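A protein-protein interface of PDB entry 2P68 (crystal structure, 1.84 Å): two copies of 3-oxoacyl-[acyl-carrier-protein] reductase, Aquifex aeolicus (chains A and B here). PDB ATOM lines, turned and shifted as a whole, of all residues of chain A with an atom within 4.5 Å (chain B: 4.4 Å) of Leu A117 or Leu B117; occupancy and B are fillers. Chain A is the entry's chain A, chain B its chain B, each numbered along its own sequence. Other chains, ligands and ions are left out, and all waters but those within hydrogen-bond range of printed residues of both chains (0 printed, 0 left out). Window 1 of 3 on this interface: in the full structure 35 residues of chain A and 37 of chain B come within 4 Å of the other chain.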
ATOM      1  N   TRP A 109     -26.644 -10.467  17.831  1.00  0.00           N
ATOM      2  CA  TRP A 109     -25.823 -11.673  17.983  1.00  0.00           C
ATOM      3  C   TRP A 109     -26.447 -12.653  18.985  1.00  0.00           C
ATOM      4  O   TRP A 109     -26.685 -13.823  18.658  1.00  0.00           O
ATOM      5  CB  TRP A 109     -24.394 -11.288  18.396  1.00  0.00           C
ATOM      6  CG  TRP A 109     -23.519 -12.466  18.741  1.00  0.00           C
ATOM      7  CD1 TRP A 109     -23.363 -13.027  19.980  1.00  0.00           C
ATOM      8  CD2 TRP A 109     -22.706 -13.229  17.851  1.00  0.00           C
ATOM      9  NE1 TRP A 109     -22.499 -14.089  19.913  1.00  0.00           N
ATOM     10  CE2 TRP A 109     -22.074 -14.234  18.620  1.00  0.00           C
ATOM     11  CE3 TRP A 109     -22.428 -13.158  16.477  1.00  0.00           C
ATOM     12  CZ2 TRP A 109     -21.196 -15.163  18.063  1.00  0.00           C
ATOM     13  CZ3 TRP A 109     -21.559 -14.089  15.926  1.00  0.00           C
ATOM     14  CH2 TRP A 109     -20.955 -15.080  16.718  1.00  0.00           C
ATOM     15  N   VAL A 112     -29.779 -14.628  18.152  1.00  0.00           N
ATOM     16  CA  VAL A 112     -29.594 -15.673  17.148  1.00  0.00           C
ATOM     17  C   VAL A 112     -28.995 -16.920  17.798  1.00  0.00           C
ATOM     18  O   VAL A 112     -29.468 -18.032  17.554  1.00  0.00           O
ATOM     19  CB  VAL A 112     -28.779 -15.167  15.919  1.00  0.00           C
ATOM     20  CG1 VAL A 112     -28.385 -16.320  14.982  1.00  0.00           C
ATOM     21  CG2 VAL A 112     -29.587 -14.135  15.148  1.00  0.00           C
ATOM     22  N   LEU A 113     -27.976 -16.734  18.643  1.00  0.00           N
ATOM     23  CA  LEU A 113     -27.421 -17.849  19.426  1.00  0.00           C
ATOM     24  C   LEU A 113     -28.447 -18.433  20.402  1.00  0.00           C
ATOM     25  O   LEU A 113     -28.539 -19.647  20.555  1.00  0.00           O
ATOM     26  CB  LEU A 113     -26.150 -17.426  20.191  1.00  0.00           C
ATOM     27  CG  LEU A 113     -24.817 -17.515  19.445  1.00  0.00           C
ATOM     28  CD1 LEU A 113     -24.813 -16.633  18.193  1.00  0.00           C
ATOM     29  CD2 LEU A 113     -23.647 -17.169  20.376  1.00  0.00           C
ATOM     30  N   VAL A 115     -31.767 -18.560  20.274  1.00  0.00           N
ATOM     31  CA  VAL A 115     -32.787 -19.383  19.608  1.00  0.00           C
ATOM     32  C   VAL A 115     -32.161 -20.600  18.935  1.00  0.00           C
ATOM     33  O   VAL A 115     -32.561 -21.739  19.209  1.00  0.00           O
ATOM     34  CB  VAL A 115     -33.608 -18.583  18.559  1.00  0.00           C
ATOM     35  CG1 VAL A 115     -34.544 -19.518  17.768  1.00  0.00           C
ATOM     36  CG2 VAL A 115     -34.419 -17.475  19.253  1.00  0.00           C
ATOM     37  N   ASN A 116     -31.189 -20.353  18.058  1.00  0.00           N
ATOM     38  CA  ASN A 116     -30.676 -21.406  17.169  1.00  0.00           C
ATOM     39  C   ASN A 116     -29.857 -22.488  17.865  1.00  0.00           C
ATOM     40  O   ASN A 116     -29.922 -23.655  17.485  1.00  0.00           O
ATOM     41  CB  ASN A 116     -29.889 -20.795  15.999  1.00  0.00           C
ATOM     42  CG  ASN A 116     -30.742 -19.849  15.137  1.00  0.00           C
ATOM     43  OD1 ASN A 116     -31.910 -19.587  15.446  1.00  0.00           O
ATOM     44  ND2 ASN A 116     -30.160 -19.341  14.057  1.00  0.00           N
ATOM     45  N   LEU A 117     -29.087 -22.094  18.879  1.00  0.00           N
ATOM     46  CA  LEU A 117     -28.236 -23.024  19.614  1.00  0.00           C
ATOM     47  C   LEU A 117     -28.834 -23.391  20.969  1.00  0.00           C
ATOM     48  O   LEU A 117     -29.078 -24.554  21.238  1.00  0.00           O
ATOM     49  CB  LEU A 117     -26.826 -22.437  19.789  1.00  0.00           C
ATOM     50  CG  LEU A 117     -26.034 -22.240  18.486  1.00  0.00           C
ATOM     51  CD1 LEU A 117     -24.621 -21.748  18.799  1.00  0.00           C
ATOM     52  CD2 LEU A 117     -25.992 -23.526  17.699  1.00  0.00           C
ATOM     53  N   THR A 118     -29.097 -22.401  21.811  1.00  0.00           N
ATOM     54  CA  THR A 118     -29.572 -22.697  23.169  1.00  0.00           C
ATOM     55  C   THR A 118     -30.997 -23.267  23.138  1.00  0.00           C
ATOM     56  O   THR A 118     -31.304 -24.208  23.862  1.00  0.00           O
ATOM     57  CB  THR A 118     -29.454 -21.479  24.074  1.00  0.00           C
ATOM     58  OG1 THR A 118     -28.072 -21.085  24.136  1.00  0.00           O
ATOM     59  CG2 THR A 118     -29.967 -21.793  25.512  1.00  0.00           C
ATOM     60  N   GLY A 119     -31.847 -22.699  22.291  1.00  0.00           N
ATOM     61  CA  GLY A 119     -33.195 -23.250  22.063  1.00  0.00           C
ATOM     62  C   GLY A 119     -33.159 -24.706  21.633  1.00  0.00           C
ATOM     63  O   GLY A 119     -33.905 -25.541  22.154  1.00  0.00           O
ATOM     64  N   THR A 120     -32.303 -25.017  20.662  1.00  0.00           N
ATOM     65  CA  THR A 120     -32.090 -26.397  20.233  1.00  0.00           C
ATOM     66  C   THR A 120     -31.607 -27.286  21.381  1.00  0.00           C
ATOM     67  O   THR A 120     -32.159 -28.365  21.609  1.00  0.00           O
ATOM     68  CB  THR A 120     -31.128 -26.448  19.031  1.00  0.00           C
ATOM     69  OG1 THR A 120     -31.758 -25.803  17.921  1.00  0.00           O
ATOM     70  CG2 THR A 120     -30.786 -27.873  18.641  1.00  0.00           C
ATOM     71  N   PHE A 121     -30.594 -26.821  22.111  1.00  0.00           N
ATOM     72  CA  PHE A 121     -30.144 -27.530  23.313  1.00  0.00           C
ATOM     73  C   PHE A 121     -31.310 -27.854  24.268  1.00  0.00           C
ATOM     74  O   PHE A 121     -31.479 -29.016  24.693  1.00  0.00           O
ATOM     75  CB  PHE A 121     -29.065 -26.714  24.030  1.00  0.00           C
ATOM     76  CG  PHE A 121     -28.769 -27.188  25.420  1.00  0.00           C
ATOM     77  CD1 PHE A 121     -27.971 -28.304  25.629  1.00  0.00           C
ATOM     78  CD2 PHE A 121     -29.280 -26.509  26.525  1.00  0.00           C
ATOM     79  CE1 PHE A 121     -27.675 -28.743  26.922  1.00  0.00           C
ATOM     80  CE2 PHE A 121     -28.993 -26.944  27.825  1.00  0.00           C
ATOM     81  CZ  PHE A 121     -28.196 -28.066  28.017  1.00  0.00           C
ATOM     82  N   THR A 159     -22.559 -18.776  12.170  1.00  0.00           N
ATOM     83  CA  THR A 159     -21.969 -19.345  13.395  1.00  0.00           C
ATOM     84  C   THR A 159     -22.885 -20.422  13.997  1.00  0.00           C
ATOM     85  O   THR A 159     -22.422 -21.497  14.373  1.00  0.00           O
ATOM     86  CB  THR A 159     -21.633 -18.233  14.410  1.00  0.00           C
ATOM     87  OG1 THR A 159     -20.597 -17.415  13.861  1.00  0.00           O
ATOM     88  CG2 THR A 159     -21.157 -18.802  15.771  1.00  0.00           C
ATOM     89  N   THR A 160     -24.180 -20.131  14.087  1.00  0.00           N
ATOM     90  CA  THR A 160     -25.118 -21.099  14.679  1.00  0.00           C
ATOM     91  C   THR A 160     -25.344 -22.315  13.790  1.00  0.00           C
ATOM     92  O   THR A 160     -25.427 -23.450  14.280  1.00  0.00           O
ATOM     93  CB  THR A 160     -26.478 -20.474  15.077  1.00  0.00           C
ATOM     94  OG1 THR A 160     -27.221 -20.108  13.902  1.00  0.00           O
ATOM     95  CG2 THR A 160     -26.281 -19.260  16.000  1.00  0.00           C
ATOM     96  N   GLY A 163     -22.325 -24.314  14.122  1.00  0.00           N
ATOM     97  CA  GLY A 163     -22.342 -24.859  15.480  1.00  0.00           C
ATOM     98  C   GLY A 163     -23.251 -26.068  15.639  1.00  0.00           C
ATOM     99  O   GLY A 163     -22.931 -27.009  16.379  1.00  0.00           O
ATOM    100  N   LEU A 164     -24.374 -26.062  14.927  1.00  0.00           N
ATOM    101  CA  LEU A 164     -25.313 -27.193  14.951  1.00  0.00           C
ATOM    102  C   LEU A 164     -24.693 -28.475  14.411  1.00  0.00           C
ATOM    103  O   LEU A 164     -25.152 -29.576  14.726  1.00  0.00           O
ATOM    104  CB  LEU A 164     -26.596 -26.855  14.179  1.00  0.00           C
ATOM    105  CG  LEU A 164     -27.537 -25.904  14.928  1.00  0.00           C
ATOM    106  CD1 LEU A 164     -28.671 -25.446  14.007  1.00  0.00           C
ATOM    107  CD2 LEU A 164     -28.097 -26.578  16.174  1.00  0.00           C
ATOM    108  N   TRP B 109     -23.935 -25.175  29.619  1.00  0.00           N
ATOM    109  CA  TRP B 109     -24.070 -24.823  28.201  1.00  0.00           C
ATOM    110  C   TRP B 109     -23.822 -23.338  27.928  1.00  0.00           C
ATOM    111  O   TRP B 109     -22.972 -22.975  27.101  1.00  0.00           O
ATOM    112  CB  TRP B 109     -25.467 -25.218  27.713  1.00  0.00           C
ATOM    113  CG  TRP B 109     -25.787 -24.763  26.324  1.00  0.00           C
ATOM    114  CD1 TRP B 109     -26.406 -23.599  25.963  1.00  0.00           C
ATOM    115  CD2 TRP B 109     -25.535 -25.479  25.111  1.00  0.00           C
ATOM    116  NE1 TRP B 109     -26.541 -23.542  24.595  1.00  0.00           N
ATOM    117  CE2 TRP B 109     -26.013 -24.682  24.050  1.00  0.00           C
ATOM    118  CE3 TRP B 109     -24.945 -26.716  24.817  1.00  0.00           C
ATOM    119  CZ2 TRP B 109     -25.921 -25.080  22.719  1.00  0.00           C
ATOM    120  CZ3 TRP B 109     -24.846 -27.109  23.485  1.00  0.00           C
ATOM    121  CH2 TRP B 109     -25.346 -26.302  22.457  1.00  0.00           C
ATOM    122  N   VAL B 112     -20.270 -21.649  28.294  1.00  0.00           N
ATOM    123  CA  VAL B 112     -19.342 -22.050  27.221  1.00  0.00           C
ATOM    124  C   VAL B 112     -19.626 -21.268  25.931  1.00  0.00           C
ATOM    125  O   VAL B 112     -18.704 -20.745  25.299  1.00  0.00           O
ATOM    126  CB  VAL B 112     -19.381 -23.571  27.000  1.00  0.00           C
ATOM    127  CG1 VAL B 112     -18.610 -23.983  25.736  1.00  0.00           C
ATOM    128  CG2 VAL B 112     -18.795 -24.280  28.214  1.00  0.00           C
ATOM    129  N   LEU B 113     -20.898 -21.165  25.553  1.00  0.00           N
ATOM    130  CA  LEU B 113     -21.267 -20.313  24.405  1.00  0.00           C
ATOM    131  C   LEU B 113     -20.891 -18.850  24.625  1.00  0.00           C
ATOM    132  O   LEU B 113     -20.364 -18.195  23.725  1.00  0.00           O
ATOM    133  CB  LEU B 113     -22.766 -20.424  24.090  1.00  0.00           C
ATOM    134  CG  LEU B 113     -23.194 -21.584  23.188  1.00  0.00           C
ATOM    135  CD1 LEU B 113     -22.909 -22.976  23.808  1.00  0.00           C
ATOM    136  CD2 LEU B 113     -24.682 -21.436  22.817  1.00  0.00           C
ATOM    137  N   VAL B 115     -18.606 -17.365  26.494  1.00  0.00           N
ATOM    138  CA  VAL B 115     -17.176 -17.107  26.433  1.00  0.00           C
ATOM    139  C   VAL B 115     -16.662 -17.392  25.028  1.00  0.00           C
ATOM    140  O   VAL B 115     -16.058 -16.519  24.394  1.00  0.00           O
ATOM    141  CB  VAL B 115     -16.380 -17.970  27.456  1.00  0.00           C
ATOM    142  CG1 VAL B 115     -14.874 -17.779  27.282  1.00  0.00           C
ATOM    143  CG2 VAL B 115     -16.815 -17.645  28.899  1.00  0.00           C
ATOM    144  N   ASN B 116     -16.898 -18.616  24.556  1.00  0.00           N
ATOM    145  CA  ASN B 116     -16.228 -19.118  23.349  1.00  0.00           C
ATOM    146  C   ASN B 116     -16.760 -18.493  22.059  1.00  0.00           C
ATOM    147  O   ASN B 116     -16.006 -18.291  21.110  1.00  0.00           O
ATOM    148  CB  ASN B 116     -16.292 -20.658  23.274  1.00  0.00           C
ATOM    149  CG  ASN B 116     -15.579 -21.353  24.446  1.00  0.00           C
ATOM    150  OD1 ASN B 116     -15.100 -20.716  25.382  1.00  0.00           O
ATOM    151  ND2 ASN B 116     -15.513 -22.668  24.383  1.00  0.00           N
ATOM    152  N   LEU B 117     -18.051 -18.181  22.024  1.00  0.00           N
ATOM    153  CA  LEU B 117     -18.644 -17.549  20.838  1.00  0.00           C
ATOM    154  C   LEU B 117     -18.854 -16.042  21.019  1.00  0.00           C
ATOM    155  O   LEU B 117     -18.307 -15.240  20.254  1.00  0.00           O
ATOM    156  CB  LEU B 117     -19.967 -18.250  20.435  1.00  0.00           C
ATOM    157  CG  LEU B 117     -19.806 -19.712  19.976  1.00  0.00           C
ATOM    158  CD1 LEU B 117     -21.148 -20.325  19.566  1.00  0.00           C
ATOM    159  CD2 LEU B 117     -18.812 -19.806  18.836  1.00  0.00           C
ATOM    160  N   THR B 118     -19.633 -15.661  22.027  1.00  0.00           N
ATOM    161  CA  THR B 118     -20.003 -14.245  22.218  1.00  0.00           C
ATOM    162  C   THR B 118     -18.789 -13.374  22.614  1.00  0.00           C
ATOM    163  O   THR B 118     -18.635 -12.251  22.124  1.00  0.00           O
ATOM    164  CB  THR B 118     -21.203 -14.096  23.176  1.00  0.00           C
ATOM    165  OG1 THR B 118     -22.307 -14.875  22.681  1.00  0.00           O
ATOM    166  CG2 THR B 118     -21.650 -12.624  23.289  1.00  0.00           C
ATOM    167  N   GLY B 119     -17.924 -13.909  23.473  1.00  0.00           N
ATOM    168  CA  GLY B 119     -16.669 -13.229  23.835  1.00  0.00           C
ATOM    169  C   GLY B 119     -15.810 -12.981  22.609  1.00  0.00           C
ATOM    170  O   GLY B 119     -15.298 -11.876  22.392  1.00  0.00           O
ATOM    171  N   THR B 120     -15.657 -14.021  21.796  1.00  0.00           N
ATOM    172  CA  THR B 120     -14.945 -13.923  20.527  1.00  0.00           C
ATOM    173  C   THR B 120     -15.544 -12.850  19.616  1.00  0.00           C
ATOM    174  O   THR B 120     -14.820 -12.034  19.031  1.00  0.00           O
ATOM    175  CB  THR B 120     -14.953 -15.288  19.844  1.00  0.00           C
ATOM    176  OG1 THR B 120     -14.381 -16.237  20.746  1.00  0.00           O
ATOM    177  CG2 THR B 120     -14.166 -15.276  18.546  1.00  0.00           C
ATOM    178  N   PHE B 121     -16.873 -12.859  19.508  1.00  0.00           N
ATOM    179  CA  PHE B 121     -17.607 -11.846  18.743  1.00  0.00           C
ATOM    180  C   PHE B 121     -17.239 -10.429  19.182  1.00  0.00           C
ATOM    181  O   PHE B 121     -16.801  -9.612  18.368  1.00  0.00           O
ATOM    182  CB  PHE B 121     -19.117 -12.088  18.897  1.00  0.00           C
ATOM    183  CG  PHE B 121     -19.979 -10.935  18.435  1.00  0.00           C
ATOM    184  CD1 PHE B 121     -20.125 -10.655  17.075  1.00  0.00           C
ATOM    185  CD2 PHE B 121     -20.664 -10.148  19.357  1.00  0.00           C
ATOM    186  CE1 PHE B 121     -20.929  -9.596  16.648  1.00  0.00           C
ATOM    187  CE2 PHE B 121     -21.473  -9.079  18.940  1.00  0.00           C
ATOM    188  CZ  PHE B 121     -21.604  -8.808  17.584  1.00  0.00           C
ATOM    189  N   THR B 159     -19.930 -27.672  19.924  1.00  0.00           N
ATOM    190  CA  THR B 159     -20.820 -26.678  19.297  1.00  0.00           C
ATOM    191  C   THR B 159     -20.082 -25.344  19.073  1.00  0.00           C
ATOM    192  O   THR B 159     -20.125 -24.776  17.968  1.00  0.00           O
ATOM    193  CB  THR B 159     -22.121 -26.475  20.113  1.00  0.00           C
ATOM    194  OG1 THR B 159     -22.896 -27.686  20.081  1.00  0.00           O
ATOM    195  CG2 THR B 159     -22.976 -25.327  19.543  1.00  0.00           C
ATOM    196  N   THR B 160     -19.394 -24.853  20.101  1.00  0.00           N
ATOM    197  CA  THR B 160     -18.677 -23.572  19.962  1.00  0.00           C
ATOM    198  C   THR B 160     -17.533 -23.673  18.959  1.00  0.00           C
ATOM    199  O   THR B 160     -17.345 -22.771  18.137  1.00  0.00           O
ATOM    200  CB  THR B 160     -18.182 -22.976  21.306  1.00  0.00           C
ATOM    201  OG1 THR B 160     -17.155 -23.804  21.874  1.00  0.00           O
ATOM    202  CG2 THR B 160     -19.357 -22.839  22.284  1.00  0.00           C
ATOM    203  N   GLY B 163     -18.969 -23.839  15.610  1.00  0.00           N
ATOM    204  CA  GLY B 163     -19.529 -22.518  15.326  1.00  0.00           C
ATOM    205  C   GLY B 163     -18.471 -21.522  14.870  1.00  0.00           C
ATOM    206  O   GLY B 163     -18.712 -20.713  13.966  1.00  0.00           O
ATOM    207  N   LEU B 164     -17.295 -21.586  15.490  1.00  0.00           N
ATOM    208  CA  LEU B 164     -16.184 -20.695  15.123  1.00  0.00           C
ATOM    209  C   LEU B 164     -15.777 -20.864  13.649  1.00  0.00           C
ATOM    210  O   LEU B 164     -15.198 -19.954  13.059  1.00  0.00           O
ATOM    211  CB  LEU B 164     -14.970 -20.917  16.049  1.00  0.00           C
ATOM    212  CG  LEU B 164     -15.046 -20.275  17.452  1.00  0.00           C
ATOM    213  CD1 LEU B 164     -13.845 -20.670  18.300  1.00  0.00           C
ATOM    214  CD2 LEU B 164     -15.133 -18.763  17.356  1.00  0.00           C
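The indole nitrogen (NE1) of Trp B109 lies within hydrogen-bond range of the side-chain hydroxyl (OG1) of Thr A118 (2.9 Å).
The indole nitrogen of Trp A109 is in hydrogen-bond range of the side-chain hydroxyl of Thr B118, 2.9 Å away.
O of Leu A113 sits at hydrogen-bond distance from N of Thr A118 (3.1 Å).
The backbone NH (N) of Thr B118 is in hydrogen-bond range of the backbone carbonyl oxygen (O) of Leu B113 (3.1 Å).
Among the printed residues, pairs that only touch across the chains: Trp A109 with Leu B117, Trp A109 with Phe B121, Leu A113 with Leu B117, Leu A113 with Thr B118, Leu A117 with Trp B109, Leu A117 with Leu B113, Leu A117 with Leu B117, Leu A117 with Thr B159, Thr A118 with Leu B113, Phe A121 with Trp B109, Thr A159 with Leu B117, Thr A159 with Gly B163, Gly A163 with Thr B159 and Gly A163 with Gly B163.
Of chain B, only Trp B109, Leu B113, Leu B117 and Thr B159 come within 4 Å of Leu A117.
Of the printed residues of chain B, Thr A118 touches Trp B109 and Leu B113.
Printed residues of chain B within 4 Å of Phe A121: Trp B109 (3.5 Å).
Printed residues of chain A within 4 Å of Thr B118: Trp A109 and Leu A113.
Of the 14 printed residues of chain A, 7 touch a printed residue of chain B.
Of the 14 printed residues of chain B, 7 touch a printed residue of chain A.
Printed residues of chain B that touch a printed residue of chain A: Trp B109, Leu B113, Leu B117, Thr B118, Phe B121, Thr B159 and Gly B163.
Trp A109 touches Leu B117, and with the chains exchanged Leu A117 touches Trp B109.
Trp A109 touches Thr B118, and with the chains exchanged Thr A118 touches Trp B109.
Leu A113 touches Leu B117, and with the chains exchanged Leu A117 touches Leu B113.
Leu A113 touches Thr B118, and with the chains exchanged Thr A118 touches Leu B113.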
